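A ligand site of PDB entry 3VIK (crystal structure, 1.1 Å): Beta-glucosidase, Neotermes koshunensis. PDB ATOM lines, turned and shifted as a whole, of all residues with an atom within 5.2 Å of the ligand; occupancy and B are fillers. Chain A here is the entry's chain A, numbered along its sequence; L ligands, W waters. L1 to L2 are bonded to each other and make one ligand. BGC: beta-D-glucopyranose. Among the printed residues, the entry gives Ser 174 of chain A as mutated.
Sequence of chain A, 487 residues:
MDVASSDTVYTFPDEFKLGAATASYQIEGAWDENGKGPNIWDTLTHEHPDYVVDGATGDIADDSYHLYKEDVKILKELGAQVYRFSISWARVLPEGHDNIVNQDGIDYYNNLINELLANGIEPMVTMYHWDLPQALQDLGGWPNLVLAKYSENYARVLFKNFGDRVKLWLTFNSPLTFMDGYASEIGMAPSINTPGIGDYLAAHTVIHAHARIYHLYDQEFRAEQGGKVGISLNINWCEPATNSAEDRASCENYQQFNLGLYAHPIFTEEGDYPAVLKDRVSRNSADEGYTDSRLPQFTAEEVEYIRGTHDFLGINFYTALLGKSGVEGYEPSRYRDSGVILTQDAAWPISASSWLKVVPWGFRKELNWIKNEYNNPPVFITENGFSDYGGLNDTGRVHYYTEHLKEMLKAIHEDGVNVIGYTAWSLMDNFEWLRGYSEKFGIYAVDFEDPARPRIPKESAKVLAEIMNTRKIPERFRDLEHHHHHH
The side-chain hydroxyl of Ser 174 is in hydrogen-bond range of an oxygen (O3) of BGC L2 (2.9 Å). OH of Tyr 318 lies within hydrogen-bond range of O4 of BGC L2, at 2.9 Å. An oxygen (O6) of BGC L2 is in hydrogen-bond range of the side-chain carboxylate (OE2) of Glu 432 (2.6 Å). OD1 of Asn 236 is in hydrogen-bond range of O6 of BGC L1 (2.9 Å). OG1 of Thr 177 is in hydrogen-bond range of O2 of BGC L2, at 2.9 Å. An oxygen (O6) of BGC L1 lies within hydrogen-bond range of the side-chain amide nitrogen of Asn 234 (3.0 Å). The side-chain carboxylate of Glu 383 lies within hydrogen-bond range of an oxygen (O3) of BGC L2, at 2.7 Å.
OH of Tyr 318 is in hydrogen-bond range of OE1 of Glu 383 (2.7 Å). The side-chain hydroxyl (OG1) of Thr 177 lies within hydrogen-bond range of the side-chain amide nitrogen (ND2) of Asn 234 (3.2 Å). The indole nitrogen (NE1) of Trp 433 sits close to the side-chain amide nitrogen (NE2) of Gln 26 (3.3 Å). The backbone carbonyl oxygen (O) of Asn 173 sits at hydrogen-bond distance from the indole nitrogen (NE1) of Trp 130 (2.9 Å). The side-chain amide nitrogen of Asn 173 lies close to a ring nitrogen (NE2) of His 129 (3.1 Å). ND2 of Asn 316 sits close to N of Glu 383. The side-chain carboxylate (OE2) of Glu 383 is in hydrogen-bond range of the side-chain amide nitrogen (ND2) of Asn 173 (2.9 Å). The side-chain amide oxygen (OD1) of Asn 173 sits close to the side-chain amide oxygen (OD1) of Asn 316, at 3.0 Å.
Merely in contact with the ligand: Trp 130, Asn 173, Trp 355, Trp 425 and Trp 433. Hydrophobic or aromatic side chains within 4 Å of the ligand: Trp 130, Tyr 318, Trp 355, Trp 425 and Trp 433. 12 residues have an atom within 4 Å of the ligand: Trp 130, Asn 173, Ser 174, Thr 177, Asn 234, Asn 236, Tyr 318, Trp 355, Glu 383, Trp 425, Glu 432 and Trp 433.
Water W5 lies within hydrogen-bond range of OE1 of Gln 26, O4 of BGC L2, NE2 of His 129 and NE1 of Trp 433. Water W7 lies within hydrogen-bond range of O1 of BGC L1 (2.8 Å) and O of Trp 355 (2.8 Å). Water W2 lies within hydrogen-bond range of the side-chain carboxylate of Glu 432 (2.6 Å), the indole nitrogen of Trp 425 (2.8 Å), an oxygen (O6) of BGC L2 (3.0 Å) and the side-chain amide nitrogen of Gln 26 (3.0 Å). Water W3 bridges ND2 of Asn 234 (3.3 Å) and O6 of BGC L1 (3.4 Å).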
ATOM      1  N   GLN A  26      33.795  -1.189 -22.357  1.00  0.00           N
ATOM      2  CA  GLN A  26      33.680  -1.138 -23.811  1.00  0.00           C
ATOM      3  C   GLN A  26      33.614   0.278 -24.353  1.00  0.00           C
ATOM      4  O   GLN A  26      33.956   0.484 -25.526  1.00  0.00           O
ATOM      5  CB  GLN A  26      32.477  -1.979 -24.263  1.00  0.00           C
ATOM      6  CG  GLN A  26      32.638  -3.426 -23.831  1.00  0.00           C
ATOM      7  CD  GLN A  26      31.587  -4.309 -24.444  1.00  0.00           C
ATOM      8  OE1 GLN A  26      30.589  -4.639 -23.799  1.00  0.00           O
ATOM      9  NE2 GLN A  26      31.809  -4.703 -25.697  1.00  0.00           N
ATOM     10  N   HIS A 129      29.677  -5.737 -15.338  1.00  0.00           N
ATOM     11  CA  HIS A 129      29.805  -6.152 -16.726  1.00  0.00           C
ATOM     12  C   HIS A 129      31.287  -6.389 -17.041  1.00  0.00           C
ATOM     13  O   HIS A 129      31.838  -5.847 -17.993  1.00  0.00           O
ATOM     14  CB  HIS A 129      29.098  -5.153 -17.652  1.00  0.00           C
ATOM     15  CG  HIS A 129      28.775  -5.660 -19.018  1.00  0.00           C
ATOM     16  ND1 HIS A 129      27.609  -5.308 -19.673  1.00  0.00           N
ATOM     17  CD2 HIS A 129      29.471  -6.445 -19.875  1.00  0.00           C
ATOM     18  CE1 HIS A 129      27.601  -5.864 -20.870  1.00  0.00           C
ATOM     19  NE2 HIS A 129      28.719  -6.539 -21.028  1.00  0.00           N
ATOM     20  N   TRP A 130      31.917  -7.237 -16.219  1.00  0.00           N
ATOM     21  CA  TRP A 130      33.139  -8.002 -16.531  1.00  0.00           C
ATOM     22  C   TRP A 130      34.429  -7.320 -16.087  1.00  0.00           C
ATOM     23  O   TRP A 130      35.487  -7.933 -16.219  1.00  0.00           O
ATOM     24  CB  TRP A 130      33.246  -8.371 -18.010  1.00  0.00           C
ATOM     25  CG  TRP A 130      32.082  -9.095 -18.596  1.00  0.00           C
ATOM     26  CD1 TRP A 130      30.880  -9.428 -18.013  1.00  0.00           C
ATOM     27  CD2 TRP A 130      32.014  -9.554 -19.949  1.00  0.00           C
ATOM     28  NE1 TRP A 130      30.085 -10.087 -18.940  1.00  0.00           N
ATOM     29  CE2 TRP A 130      30.754 -10.153 -20.134  1.00  0.00           C
ATOM     30  CE3 TRP A 130      32.917  -9.513 -21.022  1.00  0.00           C
ATOM     31  CZ2 TRP A 130      30.372 -10.730 -21.350  1.00  0.00           C
ATOM     32  CZ3 TRP A 130      32.555 -10.099 -22.222  1.00  0.00           C
ATOM     33  CH2 TRP A 130      31.278 -10.670 -22.382  1.00  0.00           C
ATOM     34  N   ASN A 173      25.991  -9.167 -15.488  1.00  0.00           N
ATOM     35  CA  ASN A 173      25.724  -9.342 -16.909  1.00  0.00           C
ATOM     36  C   ASN A 173      26.458 -10.550 -17.475  1.00  0.00           C
ATOM     37  O   ASN A 173      27.692 -10.600 -17.428  1.00  0.00           O
ATOM     38  CB  ASN A 173      26.124  -8.095 -17.687  1.00  0.00           C
ATOM     39  CG  ASN A 173      25.588  -8.150 -19.093  1.00  0.00           C
ATOM     40  OD1 ASN A 173      24.380  -7.969 -19.297  1.00  0.00           O
ATOM     41  ND2 ASN A 173      26.440  -8.454 -20.066  1.00  0.00           N
ATOM     42  N   SER A 174      25.711 -11.474 -18.078  1.00  0.00           N
ATOM     43  CA  SER A 174      26.293 -12.610 -18.784  1.00  0.00           C
ATOM     44  C   SER A 174      27.382 -13.366 -18.006  1.00  0.00           C
ATOM     45  O   SER A 174      28.483 -13.579 -18.507  1.00  0.00           O
ATOM     46  CB  SER A 174      26.838 -12.182 -20.149  1.00  0.00           C
ATOM     47  OG  SER A 174      25.774 -11.705 -20.975  1.00  0.00           O
ATOM     48  N   THR A 177      29.152 -16.187 -19.747  1.00  0.00           N
ATOM     49  CA  THR A 177      30.315 -15.777 -20.547  1.00  0.00           C
ATOM     50  C   THR A 177      31.518 -15.451 -19.656  1.00  0.00           C
ATOM     51  O   THR A 177      32.608 -15.979 -19.884  1.00  0.00           O
ATOM     52  CB  THR A 177      29.979 -14.601 -21.466  1.00  0.00           C
ATOM     53  OG1 THR A 177      28.847 -14.947 -22.278  1.00  0.00           O
ATOM     54  CG2 THR A 177      31.163 -14.236 -22.353  1.00  0.00           C
ATOM     55  N   MET A 188      39.144 -14.631 -22.295  1.00  0.00           N
ATOM     56  CA  MET A 188      38.533 -13.517 -21.554  1.00  0.00           C
ATOM     57  C   MET A 188      39.263 -13.278 -20.244  1.00  0.00           C
ATOM     58  O   MET A 188      39.657 -14.241 -19.593  1.00  0.00           O
ATOM     59  CB  MET A 188      37.077 -13.866 -21.192  1.00  0.00           C
ATOM     60  CG  MET A 188      36.081 -13.898 -22.358  1.00  0.00           C
ATOM     61  SD  MET A 188      35.649 -12.259 -23.001  1.00  0.00           S
ATOM     62  CE  MET A 188      34.404 -12.672 -24.224  1.00  0.00           C
ATOM     63  N   ASN A 234      22.808 -14.514 -20.364  1.00  0.00           N
ATOM     64  CA  ASN A 234      22.897 -14.841 -21.784  1.00  0.00           C
ATOM     65  C   ASN A 234      22.598 -16.312 -22.026  1.00  0.00           C
ATOM     66  O   ASN A 234      22.911 -17.171 -21.205  1.00  0.00           O
ATOM     67  CB  ASN A 234      24.258 -14.458 -22.378  1.00  0.00           C
ATOM     68  CG  ASN A 234      25.384 -15.303 -21.838  1.00  0.00           C
ATOM     69  OD1 ASN A 234      25.735 -15.215 -20.652  1.00  0.00           O
ATOM     70  ND2 ASN A 234      25.937 -16.166 -22.696  1.00  0.00           N
ATOM     71  N   ILE A 235      21.963 -16.593 -23.167  1.00  0.00           N
ATOM     72  CA  ILE A 235      21.621 -17.943 -23.537  1.00  0.00           C
ATOM     73  C   ILE A 235      21.385 -17.976 -25.045  1.00  0.00           C
ATOM     74  O   ILE A 235      20.675 -17.124 -25.589  1.00  0.00           O
ATOM     75  CB  ILE A 235      20.371 -18.446 -22.745  1.00  0.00           C
ATOM     76  CG1 ILE A 235      20.022 -19.903 -23.107  1.00  0.00           C
ATOM     77  CG2 ILE A 235      19.174 -17.495 -22.865  1.00  0.00           C
ATOM     78  CD1 ILE A 235      21.096 -20.937 -22.849  1.00  0.00           C
ATOM     79  N   ASN A 236      21.971 -18.996 -25.667  1.00  0.00           N
ATOM     80  CA  ASN A 236      21.723 -19.341 -27.066  1.00  0.00           C
ATOM     81  C   ASN A 236      20.589 -20.360 -27.136  1.00  0.00           C
ATOM     82  O   ASN A 236      20.526 -21.270 -26.302  1.00  0.00           O
ATOM     83  CB  ASN A 236      22.971 -19.992 -27.677  1.00  0.00           C
ATOM     84  CG  ASN A 236      24.205 -19.090 -27.689  1.00  0.00           C
ATOM     85  OD1 ASN A 236      24.088 -17.870 -27.665  1.00  0.00           O
ATOM     86  ND2 ASN A 236      25.378 -19.705 -27.690  1.00  0.00           N
ATOM     87  N   ASN A 316      20.011 -11.795 -22.371  1.00  0.00           N
ATOM     88  CA  ASN A 316      20.910 -11.391 -23.458  1.00  0.00           C
ATOM     89  C   ASN A 316      20.858 -12.500 -24.503  1.00  0.00           C
ATOM     90  O   ASN A 316      21.299 -13.628 -24.276  1.00  0.00           O
ATOM     91  CB  ASN A 316      22.329 -11.221 -22.905  1.00  0.00           C
ATOM     92  CG  ASN A 316      22.435 -10.138 -21.846  1.00  0.00           C
ATOM     93  OD1 ASN A 316      23.330 -10.162 -20.971  1.00  0.00           O
ATOM     94  ND2 ASN A 316      21.553  -9.179 -21.895  1.00  0.00           N
ATOM     95  N   TYR A 318      21.392 -13.610 -28.677  1.00  0.00           N
ATOM     96  CA  TYR A 318      22.047 -13.317 -29.957  1.00  0.00           C
ATOM     97  C   TYR A 318      21.828 -14.351 -31.051  1.00  0.00           C
ATOM     98  O   TYR A 318      21.786 -13.986 -32.237  1.00  0.00           O
ATOM     99  CB  TYR A 318      23.568 -13.183 -29.762  1.00  0.00           C
ATOM    100  CG  TYR A 318      23.972 -12.022 -28.902  1.00  0.00           C
ATOM    101  CD1 TYR A 318      24.029 -12.136 -27.520  1.00  0.00           C
ATOM    102  CD2 TYR A 318      24.256 -10.774 -29.456  1.00  0.00           C
ATOM    103  CE1 TYR A 318      24.388 -11.064 -26.715  1.00  0.00           C
ATOM    104  CE2 TYR A 318      24.621  -9.712 -28.663  1.00  0.00           C
ATOM    105  CZ  TYR A 318      24.674  -9.851 -27.280  1.00  0.00           C
ATOM    106  OH  TYR A 318      25.075  -8.763 -26.529  1.00  0.00           O
ATOM    107  N   THR A 319      21.796 -15.640 -30.720  1.00  0.00           N
ATOM    108  CA  THR A 319      21.972 -16.668 -31.736  1.00  0.00           C
ATOM    109  C   THR A 319      21.463 -18.027 -31.280  1.00  0.00           C
ATOM    110  O   THR A 319      20.939 -18.203 -30.175  1.00  0.00           O
ATOM    111  CB  THR A 319      23.453 -16.682 -32.181  1.00  0.00           C
ATOM    112  OG1 THR A 319      23.584 -17.385 -33.418  1.00  0.00           O
ATOM    113  CG2 THR A 319      24.374 -17.359 -31.154  1.00  0.00           C
ATOM    114  N   TRP A 355      30.841 -16.912 -33.808  1.00  0.00           N
ATOM    115  CA  TRP A 355      29.871 -17.551 -32.923  1.00  0.00           C
ATOM    116  C   TRP A 355      28.423 -17.130 -33.196  1.00  0.00           C
ATOM    117  O   TRP A 355      27.495 -17.756 -32.664  1.00  0.00           O
ATOM    118  CB  TRP A 355      30.256 -17.284 -31.462  1.00  0.00           C
ATOM    119  CG  TRP A 355      30.281 -15.823 -31.130  1.00  0.00           C
ATOM    120  CD1 TRP A 355      31.364 -14.995 -31.179  1.00  0.00           C
ATOM    121  CD2 TRP A 355      29.189 -15.027 -30.673  1.00  0.00           C
ATOM    122  NE1 TRP A 355      30.992 -13.722 -30.827  1.00  0.00           N
ATOM    123  CE2 TRP A 355      29.669 -13.706 -30.488  1.00  0.00           C
ATOM    124  CE3 TRP A 355      27.832 -15.286 -30.380  1.00  0.00           C
ATOM    125  CZ2 TRP A 355      28.848 -12.654 -30.061  1.00  0.00           C
ATOM    126  CZ3 TRP A 355      27.021 -14.239 -29.944  1.00  0.00           C
ATOM    127  CH2 TRP A 355      27.541 -12.944 -29.775  1.00  0.00           C
ATOM    128  N   GLU A 383      20.124  -7.327 -23.929  1.00  0.00           N
ATOM    129  CA  GLU A 383      21.003  -7.264 -25.092  1.00  0.00           C
ATOM    130  C   GLU A 383      20.374  -8.076 -26.213  1.00  0.00           C
ATOM    131  O   GLU A 383      19.928  -9.202 -25.997  1.00  0.00           O
ATOM    132  CB  GLU A 383      22.386  -7.859 -24.839  1.00  0.00           C
ATOM    133  CG  GLU A 383      23.220  -7.151 -23.791  1.00  0.00           C
ATOM    134  CD  GLU A 383      24.483  -7.868 -23.355  1.00  0.00           C
ATOM    135  OE1 GLU A 383      24.839  -8.944 -23.895  1.00  0.00           O
ATOM    136  OE2 GLU A 383      25.099  -7.357 -22.390  1.00  0.00           O
ATOM    137  N   TRP A 425      21.663  -4.002 -28.301  1.00  0.00           N
ATOM    138  CA  TRP A 425      23.118  -4.042 -28.127  1.00  0.00           C
ATOM    139  C   TRP A 425      23.772  -3.770 -29.477  1.00  0.00           C
ATOM    140  O   TRP A 425      23.628  -4.590 -30.374  1.00  0.00           O
ATOM    141  CB  TRP A 425      23.598  -5.413 -27.636  1.00  0.00           C
ATOM    142  CG  TRP A 425      25.059  -5.355 -27.341  1.00  0.00           C
ATOM    143  CD1 TRP A 425      26.084  -5.741 -28.156  1.00  0.00           C
ATOM    144  CD2 TRP A 425      25.650  -4.743 -26.194  1.00  0.00           C
ATOM    145  NE1 TRP A 425      27.285  -5.442 -27.562  1.00  0.00           N
ATOM    146  CE2 TRP A 425      27.051  -4.844 -26.355  1.00  0.00           C
ATOM    147  CE3 TRP A 425      25.145  -4.147 -25.026  1.00  0.00           C
ATOM    148  CZ2 TRP A 425      27.950  -4.364 -25.397  1.00  0.00           C
ATOM    149  CZ3 TRP A 425      26.037  -3.683 -24.067  1.00  0.00           C
ATOM    150  CH2 TRP A 425      27.420  -3.776 -24.273  1.00  0.00           C
ATOM    151  N   GLU A 432      35.170  -4.436 -28.575  1.00  0.00           N
ATOM    152  CA  GLU A 432      34.571  -5.764 -28.571  1.00  0.00           C
ATOM    153  C   GLU A 432      35.502  -6.819 -27.962  1.00  0.00           C
ATOM    154  O   GLU A 432      35.798  -7.856 -28.560  1.00  0.00           O
ATOM    155  CB  GLU A 432      34.052  -6.085 -29.984  1.00  0.00           C
ATOM    156  CG  GLU A 432      33.413  -7.469 -30.164  1.00  0.00           C
ATOM    157  CD  GLU A 432      32.334  -7.817 -29.148  1.00  0.00           C
ATOM    158  OE1 GLU A 432      31.638  -6.878 -28.701  1.00  0.00           O
ATOM    159  OE2 GLU A 432      32.200  -9.005 -28.848  1.00  0.00           O
ATOM    160  N   TRP A 433      35.894  -6.576 -26.713  1.00  0.00           N
ATOM    161  CA  TRP A 433      36.635  -7.565 -25.941  1.00  0.00           C
ATOM    162  C   TRP A 433      37.847  -8.074 -26.723  1.00  0.00           C
ATOM    163  O   TRP A 433      38.630  -7.273 -27.239  1.00  0.00           O
ATOM    164  CB  TRP A 433      35.678  -8.640 -25.406  1.00  0.00           C
ATOM    165  CG  TRP A 433      34.490  -8.066 -24.663  1.00  0.00           C
ATOM    166  CD1 TRP A 433      33.178  -8.167 -25.033  1.00  0.00           C
ATOM    167  CD2 TRP A 433      34.521  -7.290 -23.452  1.00  0.00           C
ATOM    168  NE1 TRP A 433      32.375  -7.521 -24.103  1.00  0.00           N
ATOM    169  CE2 TRP A 433      33.168  -6.982 -23.124  1.00  0.00           C
ATOM    170  CE3 TRP A 433      35.527  -6.865 -22.572  1.00  0.00           C
ATOM    171  CZ2 TRP A 433      32.816  -6.249 -21.981  1.00  0.00           C
ATOM    172  CZ3 TRP A 433      35.176  -6.134 -21.443  1.00  0.00           C
ATOM    173  CH2 TRP A 433      33.837  -5.847 -21.155  1.00  0.00           C
ATOM    174  N   PHE A 441      29.248  -3.707 -33.382  1.00  0.00           N
ATOM    175  CA  PHE A 441      27.905  -4.039 -32.912  1.00  0.00           C
ATOM    176  C   PHE A 441      27.002  -2.807 -32.791  1.00  0.00           C
ATOM    177  O   PHE A 441      25.848  -2.930 -32.383  1.00  0.00           O
ATOM    178  CB  PHE A 441      27.951  -4.754 -31.542  1.00  0.00           C
ATOM    179  CG  PHE A 441      28.189  -6.235 -31.613  1.00  0.00           C
ATOM    180  CD1 PHE A 441      27.102  -7.117 -31.709  1.00  0.00           C
ATOM    181  CD2 PHE A 441      29.469  -6.772 -31.545  1.00  0.00           C
ATOM    182  CE1 PHE A 441      27.269  -8.485 -31.760  1.00  0.00           C
ATOM    183  CE2 PHE A 441      29.654  -8.143 -31.608  1.00  0.00           C
ATOM    184  CZ  PHE A 441      28.551  -9.023 -31.706  1.00  0.00           C
HETATM  185  C2  BGC L   1      29.906 -16.842 -27.575  1.00  0.00           C
HETATM  186  C3  BGC L   1      30.010 -15.590 -26.700  1.00  0.00           C
HETATM  187  C4  BGC L   1      28.658 -14.895 -26.566  1.00  0.00           C
HETATM  188  C5  BGC L   1      27.561 -15.892 -26.171  1.00  0.00           C
HETATM  189  C6  BGC L   1      26.156 -15.303 -26.104  1.00  0.00           C
HETATM  190  C1  BGC L   1      28.755 -17.733 -27.101  1.00  0.00           C
HETATM  191  O1  BGC L   1      28.525 -18.875 -27.925  1.00  0.00           O
HETATM  192  O2  BGC L   1      31.115 -17.602 -27.526  1.00  0.00           O
HETATM  193  O3  BGC L   1      30.951 -14.689 -27.281  1.00  0.00           O
HETATM  194  O4  BGC L   1      28.821 -13.963 -25.497  1.00  0.00           O
HETATM  195  O5  BGC L   1      27.529 -17.007 -27.078  1.00  0.00           O
HETATM  196  O6  BGC L   1      25.206 -16.227 -25.573  1.00  0.00           O
HETATM  197  C2  BGC L   2      27.983 -12.109 -24.257  1.00  0.00           C
HETATM  198  C3  BGC L   2      27.357 -10.726 -24.386  1.00  0.00           C
HETATM  199  C4  BGC L   2      28.280  -9.883 -25.263  1.00  0.00           C
HETATM  200  C5  BGC L   2      28.462 -10.563 -26.618  1.00  0.00           C
HETATM  201  C6  BGC L   2      29.342  -9.851 -27.624  1.00  0.00           C
HETATM  202  C1  BGC L   2      28.196 -12.696 -25.645  1.00  0.00           C
HETATM  203  O2  BGC L   2      27.113 -12.950 -23.504  1.00  0.00           O
HETATM  204  O3  BGC L   2      27.105 -10.192 -23.076  1.00  0.00           O
HETATM  205  O4  BGC L   2      27.789  -8.553 -25.396  1.00  0.00           O
HETATM  206  O5  BGC L   2      29.044 -11.845 -26.401  1.00  0.00           O
HETATM  207  O6  BGC L   2      30.529  -9.477 -26.923  1.00  0.00           O
HETATM  208  O   HOH W   1      29.226 -21.605 -27.557  1.00  0.00           O
HETATM  209  O   HOH W   2      29.807  -6.584 -26.899  1.00  0.00           O
HETATM  210  O   HOH W   3      26.823 -18.886 -24.300  1.00  0.00           O
HETATM  211  O   HOH W   4      31.746 -19.698 -29.065  1.00  0.00           O
HETATM  212  O   HOH W   5      29.469  -7.118 -23.727  1.00  0.00           O
HETATM  213  O   HOH W   6      33.367 -15.466 -28.436  1.00  0.00           O
HETATM  214  O   HOH W   7      27.615 -19.528 -30.473  1.00  0.00           O
HETATM  215  O   HOH W   8      31.774 -12.359 -26.094  1.00  0.00           O
HETATM  216  O   HOH W   9      32.218 -17.669 -24.712  1.00  0.00           O
